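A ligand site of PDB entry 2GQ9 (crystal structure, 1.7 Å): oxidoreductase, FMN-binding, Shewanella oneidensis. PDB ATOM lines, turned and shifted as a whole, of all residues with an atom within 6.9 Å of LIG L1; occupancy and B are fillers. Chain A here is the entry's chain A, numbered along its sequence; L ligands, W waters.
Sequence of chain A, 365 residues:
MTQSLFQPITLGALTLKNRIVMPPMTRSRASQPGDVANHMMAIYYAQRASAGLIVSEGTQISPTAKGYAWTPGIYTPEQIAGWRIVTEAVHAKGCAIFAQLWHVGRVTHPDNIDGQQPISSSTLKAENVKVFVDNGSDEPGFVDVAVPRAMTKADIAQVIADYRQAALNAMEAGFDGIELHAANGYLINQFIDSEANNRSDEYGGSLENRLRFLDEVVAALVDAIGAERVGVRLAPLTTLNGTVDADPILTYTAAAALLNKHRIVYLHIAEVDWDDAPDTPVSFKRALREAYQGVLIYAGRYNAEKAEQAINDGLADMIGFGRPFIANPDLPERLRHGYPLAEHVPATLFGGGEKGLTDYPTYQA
The backbone NH (N) of Thr 26 sits at hydrogen-bond distance from a nitrogen (N3) of LG2 L2 (2.8 Å).
NH2 of Arg 233 sits at hydrogen-bond distance from O4 of LG2 L2 (2.7 Å).
An oxygen (O3) of LG2 L2 sits at hydrogen-bond distance from the backbone carbonyl oxygen (O) of Pro 24 (2.8 Å).
The side-chain amide oxygen (OE1) of Gln 100 lies within hydrogen-bond range of a nitrogen (N2) of LG2 L2 (2.8 Å).
O2 of LIG L1 sits at hydrogen-bond distance from NE2 of His 181 (2.8 Å).
The side-chain amide nitrogen (ND2) of Asn 184 is in hydrogen-bond range of an oxygen (O2) of LIG L1.
The side-chain hydroxyl of Thr 26 is in hydrogen-bond range of an oxygen (O2) of LG2 L2.
An oxygen (O1) of LG2 L2 is in hydrogen-bond range of a ring nitrogen (NE2) of His 181 (3.0 Å).
O2 of LG2 L2 lies within hydrogen-bond range of N of Gly 58 (3.1 Å).
An oxygen (O2) of LIG L1 sits close to a nitrogen (N1) of LG2 L2, at 3.2 Å.
The side-chain hydroxyl (OH) of Tyr 186 sits at hydrogen-bond distance from the side-chain amide oxygen (OD1) of Asn 241, at 3.1 Å.
OH of Tyr 68 sits at hydrogen-bond distance from OH of Tyr 186, 2.7 Å away.
ND1 of His 181 is in hydrogen-bond range of N of Ala 183, at 3.2 Å.
OD1 of Asn 241 sits close to O of Asn 184, at 2.8 Å.
Thr 26 touches LIG L1 (OG1 to C3, 3.5 Å).
Trp 102 touches LIG L1.
CE1 of Tyr 186 touches O2 of LIG L1, at 3.3 Å.
Asp 273 touches LIG L1 (OD1 to C6, 3.8 Å).
Trp 274 touches LIG L1 (CZ2 to O1, 3.3 Å).
Phe 350 touches LIG L1.
Hydrophobic or aromatic side chains within 4 Å of LIG L1: Trp 102, His 181, Tyr 186, Trp 274 and Phe 350.
Of the 18 residues printed, 8 come within 4 Å of LIG L1.
The nearest printed residue that does not touch LIG L1 is Tyr 68 (4.6 Å).
Water W1 bridges the side-chain carboxylate of Asp 273 (2.6 Å) and the side-chain amide oxygen of Asn 241 (3.4 Å).
Water W2 bridges an oxygen (O2) of LG3 L3 and an oxygen (O1) of LIG L1.
Water W3 bridges NE1 of Trp 274 (3.2 Å) and O1 of LIG L1 (3.4 Å).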
ATOM      1  N   PRO A  24      13.579 -20.793 -12.029  1.00  0.00           N
ATOM      2  CA  PRO A  24      14.842 -20.061 -12.195  1.00  0.00           C
ATOM      3  C   PRO A  24      14.879 -19.332 -13.525  1.00  0.00           C
ATOM      4  O   PRO A  24      14.661 -19.948 -14.563  1.00  0.00           O
ATOM      5  CB  PRO A  24      15.902 -21.167 -12.110  1.00  0.00           C
ATOM      6  CG  PRO A  24      15.170 -22.379 -12.609  1.00  0.00           C
ATOM      7  CD  PRO A  24      13.821 -22.247 -11.954  1.00  0.00           C
ATOM      8  N   MET A  25      15.157 -18.030 -13.483  1.00  0.00           N
ATOM      9  CA  MET A  25      15.230 -17.257 -14.718  1.00  0.00           C
ATOM     10  C   MET A  25      16.342 -16.223 -14.736  1.00  0.00           C
ATOM     11  O   MET A  25      16.295 -15.193 -14.057  1.00  0.00           O
ATOM     12  CB  MET A  25      13.893 -16.583 -15.044  1.00  0.00           C
ATOM     13  CG  MET A  25      12.809 -17.577 -15.433  1.00  0.00           C
ATOM     14  SD  MET A  25      11.256 -16.792 -15.835  1.00  0.00           S
ATOM     15  CE  MET A  25      10.778 -16.119 -14.228  1.00  0.00           C
ATOM     16  N   THR A  26      17.367 -16.534 -15.515  1.00  0.00           N
ATOM     17  CA  THR A  26      18.532 -15.679 -15.715  1.00  0.00           C
ATOM     18  C   THR A  26      18.071 -14.354 -16.299  1.00  0.00           C
ATOM     19  O   THR A  26      17.388 -14.327 -17.315  1.00  0.00           O
ATOM     20  CB  THR A  26      19.502 -16.344 -16.704  1.00  0.00           C
ATOM     21  OG1 THR A  26      20.034 -17.534 -16.099  1.00  0.00           O
ATOM     22  CG2 THR A  26      20.627 -15.403 -17.082  1.00  0.00           C
ATOM     23  N   ARG A  27      18.436 -13.248 -15.640  1.00  0.00           N
ATOM     24  CA  ARG A  27      18.075 -11.907 -16.112  1.00  0.00           C
ATOM     25  C   ARG A  27      19.348 -11.101 -16.373  1.00  0.00           C
ATOM     26  O   ARG A  27      19.282  -9.995 -16.909  1.00  0.00           O
ATOM     27  CB  ARG A  27      17.196 -11.189 -15.077  1.00  0.00           C
ATOM     28  CG  ARG A  27      15.906 -11.915 -14.704  1.00  0.00           C
ATOM     29  CD  ARG A  27      15.101 -12.329 -15.936  1.00  0.00           C
ATOM     30  NE  ARG A  27      14.726 -11.168 -16.744  1.00  0.00           N
ATOM     31  CZ  ARG A  27      13.729 -10.328 -16.469  1.00  0.00           C
ATOM     32  NH1 ARG A  27      12.955 -10.515 -15.398  1.00  0.00           N
ATOM     33  NH2 ARG A  27      13.517  -9.296 -17.260  1.00  0.00           N
ATOM     34  N   GLY A  58      19.903 -18.975 -12.262  1.00  0.00           N
ATOM     35  CA  GLY A  58      21.131 -19.722 -12.065  1.00  0.00           C
ATOM     36  C   GLY A  58      22.225 -18.816 -11.527  1.00  0.00           C
ATOM     37  O   GLY A  58      22.378 -17.666 -11.957  1.00  0.00           O
ATOM     38  N   TYR A  68      27.299 -16.900 -19.063  1.00  0.00           N
ATOM     39  CA  TYR A  68      26.751 -15.693 -19.667  1.00  0.00           C
ATOM     40  C   TYR A  68      27.165 -14.447 -18.886  1.00  0.00           C
ATOM     41  O   TYR A  68      27.320 -14.481 -17.670  1.00  0.00           O
ATOM     42  CB  TYR A  68      25.221 -15.791 -19.687  1.00  0.00           C
ATOM     43  CG  TYR A  68      24.712 -17.064 -20.329  1.00  0.00           C
ATOM     44  CD1 TYR A  68      24.397 -17.104 -21.687  1.00  0.00           C
ATOM     45  CD2 TYR A  68      24.595 -18.233 -19.587  1.00  0.00           C
ATOM     46  CE1 TYR A  68      23.959 -18.292 -22.289  1.00  0.00           C
ATOM     47  CE2 TYR A  68      24.168 -19.418 -20.176  1.00  0.00           C
ATOM     48  CZ  TYR A  68      23.856 -19.442 -21.518  1.00  0.00           C
ATOM     49  OH  TYR A  68      23.448 -20.628 -22.092  1.00  0.00           O
ATOM     50  N   GLN A 100      19.549 -21.518  -7.278  1.00  0.00           N
ATOM     51  CA  GLN A 100      19.864 -22.530  -8.280  1.00  0.00           C
ATOM     52  C   GLN A 100      21.363 -22.527  -8.536  1.00  0.00           C
ATOM     53  O   GLN A 100      21.897 -21.608  -9.167  1.00  0.00           O
ATOM     54  CB  GLN A 100      19.131 -22.300  -9.616  1.00  0.00           C
ATOM     55  CG  GLN A 100      19.409 -23.453 -10.589  1.00  0.00           C
ATOM     56  CD  GLN A 100      18.863 -23.236 -11.978  1.00  0.00           C
ATOM     57  OE1 GLN A 100      19.230 -22.288 -12.653  1.00  0.00           O
ATOM     58  NE2 GLN A 100      18.003 -24.145 -12.418  1.00  0.00           N
ATOM     59  N   TRP A 102      24.599 -23.248 -10.258  1.00  0.00           N
ATOM     60  CA  TRP A 102      24.890 -23.421 -11.675  1.00  0.00           C
ATOM     61  C   TRP A 102      26.331 -23.651 -12.100  1.00  0.00           C
ATOM     62  O   TRP A 102      27.262 -23.028 -11.579  1.00  0.00           O
ATOM     63  CB  TRP A 102      24.386 -22.157 -12.360  1.00  0.00           C
ATOM     64  CG  TRP A 102      24.093 -22.203 -13.820  1.00  0.00           C
ATOM     65  CD1 TRP A 102      23.911 -23.304 -14.614  1.00  0.00           C
ATOM     66  CD2 TRP A 102      23.798 -21.064 -14.646  1.00  0.00           C
ATOM     67  NE1 TRP A 102      23.509 -22.924 -15.874  1.00  0.00           N
ATOM     68  CE2 TRP A 102      23.437 -21.550 -15.919  1.00  0.00           C
ATOM     69  CE3 TRP A 102      23.813 -19.678 -14.423  1.00  0.00           C
ATOM     70  CZ2 TRP A 102      23.070 -20.700 -16.964  1.00  0.00           C
ATOM     71  CZ3 TRP A 102      23.453 -18.834 -15.457  1.00  0.00           C
ATOM     72  CH2 TRP A 102      23.090 -19.347 -16.716  1.00  0.00           C
ATOM     73  N   HIS A 181      21.170 -27.318 -10.720  1.00  0.00           N
ATOM     74  CA  HIS A 181      20.808 -27.191 -12.131  1.00  0.00           C
ATOM     75  C   HIS A 181      21.468 -28.340 -12.884  1.00  0.00           C
ATOM     76  O   HIS A 181      22.650 -28.264 -13.228  1.00  0.00           O
ATOM     77  CB  HIS A 181      21.291 -25.866 -12.723  1.00  0.00           C
ATOM     78  CG  HIS A 181      20.648 -25.539 -14.043  1.00  0.00           C
ATOM     79  ND1 HIS A 181      19.942 -26.466 -14.780  1.00  0.00           N
ATOM     80  CD2 HIS A 181      20.572 -24.376 -14.736  1.00  0.00           C
ATOM     81  CE1 HIS A 181      19.459 -25.897 -15.862  1.00  0.00           C
ATOM     82  NE2 HIS A 181      19.821 -24.619 -15.869  1.00  0.00           N
ATOM     83  N   ALA A 183      19.948 -29.531 -15.612  1.00  0.00           N
ATOM     84  CA  ALA A 183      19.146 -29.486 -16.821  1.00  0.00           C
ATOM     85  C   ALA A 183      19.707 -28.577 -17.904  1.00  0.00           C
ATOM     86  O   ALA A 183      20.832 -28.088 -17.837  1.00  0.00           O
ATOM     87  CB  ALA A 183      17.713 -29.042 -16.477  1.00  0.00           C
ATOM     88  N   ASN A 184      18.852 -28.374 -18.905  1.00  0.00           N
ATOM     89  CA  ASN A 184      19.095 -27.524 -20.048  1.00  0.00           C
ATOM     90  C   ASN A 184      20.467 -27.536 -20.687  1.00  0.00           C
ATOM     91  O   ASN A 184      20.979 -26.497 -21.123  1.00  0.00           O
ATOM     92  CB  ASN A 184      18.629 -26.104 -19.697  1.00  0.00           C
ATOM     93  CG  ASN A 184      17.190 -26.095 -19.212  1.00  0.00           C
ATOM     94  OD1 ASN A 184      16.456 -27.052 -19.444  1.00  0.00           O
ATOM     95  ND2 ASN A 184      16.785 -25.016 -18.543  1.00  0.00           N
ATOM     96  N   GLY A 185      21.053 -28.722 -20.768  1.00  0.00           N
ATOM     97  CA  GLY A 185      22.333 -28.888 -21.416  1.00  0.00           C
ATOM     98  C   GLY A 185      23.577 -28.349 -20.736  1.00  0.00           C
ATOM     99  O   GLY A 185      24.587 -28.137 -21.404  1.00  0.00           O
ATOM    100  N   TYR A 186      23.510 -28.115 -19.430  1.00  0.00           N
ATOM    101  CA  TYR A 186      24.670 -27.614 -18.715  1.00  0.00           C
ATOM    102  C   TYR A 186      25.563 -28.744 -18.199  1.00  0.00           C
ATOM    103  O   TYR A 186      25.366 -29.903 -18.578  1.00  0.00           O
ATOM    104  CB  TYR A 186      24.194 -26.627 -17.641  1.00  0.00           C
ATOM    105  CG  TYR A 186      23.613 -25.394 -18.321  1.00  0.00           C
ATOM    106  CD1 TYR A 186      22.272 -25.066 -18.186  1.00  0.00           C
ATOM    107  CD2 TYR A 186      24.406 -24.612 -19.170  1.00  0.00           C
ATOM    108  CE1 TYR A 186      21.716 -23.999 -18.892  1.00  0.00           C
ATOM    109  CE2 TYR A 186      23.864 -23.538 -19.881  1.00  0.00           C
ATOM    110  CZ  TYR A 186      22.518 -23.245 -19.735  1.00  0.00           C
ATOM    111  OH  TYR A 186      21.965 -22.200 -20.446  1.00  0.00           O
ATOM    112  N   ARG A 233      17.028 -30.041 -10.665  1.00  0.00           N
ATOM    113  CA  ARG A 233      16.259 -29.806 -11.880  1.00  0.00           C
ATOM    114  C   ARG A 233      16.813 -30.625 -13.040  1.00  0.00           C
ATOM    115  O   ARG A 233      18.024 -30.654 -13.267  1.00  0.00           O
ATOM    116  CB  ARG A 233      16.278 -28.318 -12.255  1.00  0.00           C
ATOM    117  CG  ARG A 233      15.148 -27.976 -13.221  1.00  0.00           C
ATOM    118  CD  ARG A 233      15.074 -26.512 -13.625  1.00  0.00           C
ATOM    119  NE  ARG A 233      13.680 -26.177 -13.946  1.00  0.00           N
ATOM    120  CZ  ARG A 233      13.278 -25.189 -14.741  1.00  0.00           C
ATOM    121  NH1 ARG A 233      14.159 -24.388 -15.310  1.00  0.00           N
ATOM    122  NH2 ARG A 233      11.990 -24.979 -14.932  1.00  0.00           N
ATOM    123  N   ASN A 241      20.113 -26.826 -25.836  1.00  0.00           N
ATOM    124  CA  ASN A 241      21.518 -26.473 -25.589  1.00  0.00           C
ATOM    125  C   ASN A 241      22.555 -27.483 -26.089  1.00  0.00           C
ATOM    126  O   ASN A 241      23.738 -27.385 -25.749  1.00  0.00           O
ATOM    127  CB  ASN A 241      21.733 -26.175 -24.104  1.00  0.00           C
ATOM    128  CG  ASN A 241      21.704 -24.679 -23.799  1.00  0.00           C
ATOM    129  OD1 ASN A 241      21.503 -24.265 -22.659  1.00  0.00           O
ATOM    130  ND2 ASN A 241      21.907 -23.863 -24.833  1.00  0.00           N
ATOM    131  N   ASP A 273      11.869 -25.396 -23.009  1.00  0.00           N
ATOM    132  CA  ASP A 273      12.992 -24.472 -22.947  1.00  0.00           C
ATOM    133  C   ASP A 273      12.792 -23.594 -24.178  1.00  0.00           C
ATOM    134  O   ASP A 273      13.097 -24.009 -25.293  1.00  0.00           O
ATOM    135  CB  ASP A 273      14.316 -25.231 -23.006  1.00  0.00           C
ATOM    136  CG  ASP A 273      15.476 -24.423 -22.446  1.00  0.00           C
ATOM    137  OD1 ASP A 273      15.267 -23.717 -21.434  1.00  0.00           O
ATOM    138  OD2 ASP A 273      16.591 -24.509 -22.996  1.00  0.00           O
ATOM    139  N   TRP A 274      12.269 -22.391 -23.950  1.00  0.00           N
ATOM    140  CA  TRP A 274      11.982 -21.457 -25.029  1.00  0.00           C
ATOM    141  C   TRP A 274      10.887 -22.046 -25.909  1.00  0.00           C
ATOM    142  O   TRP A 274       9.775 -22.287 -25.443  1.00  0.00           O
ATOM    143  CB  TRP A 274      13.250 -21.157 -25.825  1.00  0.00           C
ATOM    144  CG  TRP A 274      14.269 -20.454 -25.007  1.00  0.00           C
ATOM    145  CD1 TRP A 274      15.450 -20.952 -24.546  1.00  0.00           C
ATOM    146  CD2 TRP A 274      14.154 -19.127 -24.480  1.00  0.00           C
ATOM    147  NE1 TRP A 274      16.087 -20.018 -23.760  1.00  0.00           N
ATOM    148  CE2 TRP A 274      15.313 -18.880 -23.704  1.00  0.00           C
ATOM    149  CE3 TRP A 274      13.191 -18.113 -24.587  1.00  0.00           C
ATOM    150  CZ2 TRP A 274      15.534 -17.670 -23.042  1.00  0.00           C
ATOM    151  CZ3 TRP A 274      13.412 -16.903 -23.925  1.00  0.00           C
ATOM    152  CH2 TRP A 274      14.577 -16.700 -23.158  1.00  0.00           C
ATOM    153  N   PHE A 350      17.396  -9.817 -20.707  1.00  0.00           N
ATOM    154  CA  PHE A 350      18.754  -9.848 -20.199  1.00  0.00           C
ATOM    155  C   PHE A 350      19.487  -8.519 -20.243  1.00  0.00           C
ATOM    156  O   PHE A 350      19.358  -7.749 -21.198  1.00  0.00           O
ATOM    157  CB  PHE A 350      19.589 -10.862 -20.972  1.00  0.00           C
ATOM    158  CG  PHE A 350      18.901 -12.170 -21.198  1.00  0.00           C
ATOM    159  CD1 PHE A 350      18.297 -12.456 -22.424  1.00  0.00           C
ATOM    160  CD2 PHE A 350      18.882 -13.137 -20.201  1.00  0.00           C
ATOM    161  CE1 PHE A 350      17.683 -13.687 -22.655  1.00  0.00           C
ATOM    162  CE2 PHE A 350      18.275 -14.375 -20.422  1.00  0.00           C
ATOM    163  CZ  PHE A 350      17.674 -14.651 -21.645  1.00  0.00           C
HETATM  164  C1  LIG L   1      19.029 -18.145 -20.367  1.00  0.00           C
HETATM  165  O1  LIG L   1      18.257 -17.831 -21.255  1.00  0.00           O
HETATM  166  C2  LIG L   1      18.946 -19.463 -19.741  1.00  0.00           C
HETATM  167  C3  LIG L   1      19.852 -19.821 -18.694  1.00  0.00           C
HETATM  168  C4  LIG L   1      19.800 -21.119 -18.162  1.00  0.00           C
HETATM  169  C5  LIG L   1      18.855 -22.045 -18.659  1.00  0.00           C
HETATM  170  C6  LIG L   1      17.919 -21.722 -19.669  1.00  0.00           C
HETATM  171  C7  LIG L   1      17.979 -20.425 -20.178  1.00  0.00           C
HETATM  172  O2  LIG L   1      18.649 -23.168 -17.928  1.00  0.00           O
HETATM  173  N1  LG2 L   2      15.922 -22.379 -16.404  1.00  0.00           N
HETATM  174  C1  LG2 L   2      16.927 -22.750 -15.486  1.00  0.00           C
HETATM  175  O1  LG2 L   2      17.003 -23.867 -15.056  1.00  0.00           O
HETATM  176  N2  LG2 L   2      17.831 -21.719 -15.024  1.00  0.00           N
HETATM  177  C2  LG2 L   2      17.825 -20.408 -15.408  1.00  0.00           C
HETATM  178  O2  LG2 L   2      18.696 -19.633 -15.042  1.00  0.00           O
HETATM  179  C3  LG2 L   2      16.854 -20.024 -16.464  1.00  0.00           C
HETATM  180  N3  LG2 L   2      16.973 -18.825 -17.133  1.00  0.00           N
HETATM  181  C4  LG2 L   2      15.908 -18.446 -17.916  1.00  0.00           C
HETATM  182  C5  LG2 L   2      15.854 -17.053 -18.428  1.00  0.00           C
HETATM  183  C6  LG2 L   2      14.702 -16.544 -19.145  1.00  0.00           C
HETATM  184  C7  LG2 L   2      14.673 -15.074 -19.546  1.00  0.00           C
HETATM  185  C8  LG2 L   2      13.603 -17.463 -19.443  1.00  0.00           C
HETATM  186  C9  LG2 L   2      12.309 -16.976 -20.147  1.00  0.00           C
HETATM  187  C10 LG2 L   2      13.673 -18.833 -18.985  1.00  0.00           C
HETATM  188  C11 LG2 L   2      14.784 -19.332 -18.254  1.00  0.00           C
HETATM  189  N4  LG2 L   2      14.882 -20.668 -17.664  1.00  0.00           N
HETATM  190  C12 LG2 L   2      15.902 -21.127 -16.860  1.00  0.00           C
HETATM  191  C13 LG2 L   2      13.787 -21.649 -18.010  1.00  0.00           C
HETATM  192  C14 LG2 L   2      12.603 -21.438 -17.072  1.00  0.00           C
HETATM  193  O3  LG2 L   2      12.907 -21.730 -15.708  1.00  0.00           O
HETATM  194  C15 LG2 L   2      11.358 -22.239 -17.471  1.00  0.00           C
HETATM  195  O4  LG2 L   2      11.604 -23.650 -17.299  1.00  0.00           O
HETATM  196  C16 LG2 L   2      10.943 -21.982 -18.914  1.00  0.00           C
HETATM  197  O5  LG2 L   2      10.840 -20.550 -19.195  1.00  0.00           O
HETATM  198  C17 LG2 L   2       9.655 -22.671 -19.305  1.00  0.00           C
HETATM  199  O6  LG2 L   2       8.511 -22.119 -18.556  1.00  0.00           O
HETATM  200  P1  LG2 L   2       7.510 -21.040 -19.143  1.00  0.00           P
HETATM  201  O7  LG2 L   2       8.221 -19.734 -19.325  1.00  0.00           O
HETATM  202  O8  LG2 L   2       6.931 -21.614 -20.426  1.00  0.00           O
HETATM  203  O9  LG2 L   2       6.415 -20.910 -18.057  1.00  0.00           O
HETATM  204  C1  LG3 L   3      22.779  -9.818 -22.833  1.00  0.00           C
HETATM  205  O1  LG3 L   3      22.173  -9.564 -23.845  1.00  0.00           O
HETATM  206  C2  LG3 L   3      22.729 -11.177 -22.252  1.00  0.00           C
HETATM  207  C3  LG3 L   3      23.434 -11.466 -21.045  1.00  0.00           C
HETATM  208  C4  LG3 L   3      23.427 -12.774 -20.557  1.00  0.00           C
HETATM  209  C5  LG3 L   3      22.711 -13.793 -21.246  1.00  0.00           C
HETATM  210  C6  LG3 L   3      21.971 -13.531 -22.437  1.00  0.00           C
HETATM  211  C7  LG3 L   3      21.979 -12.210 -22.899  1.00  0.00           C
HETATM  212  O2  LG3 L   3      22.493 -14.949 -20.600  1.00  0.00           O
HETATM  213  O   HOH W   1      18.428 -22.708 -22.707  1.00  0.00           O
HETATM  214  O   HOH W   2      21.140 -16.520 -22.252  1.00  0.00           O
HETATM  215  O   HOH W   3      19.279 -20.293 -23.416  1.00  0.00           O
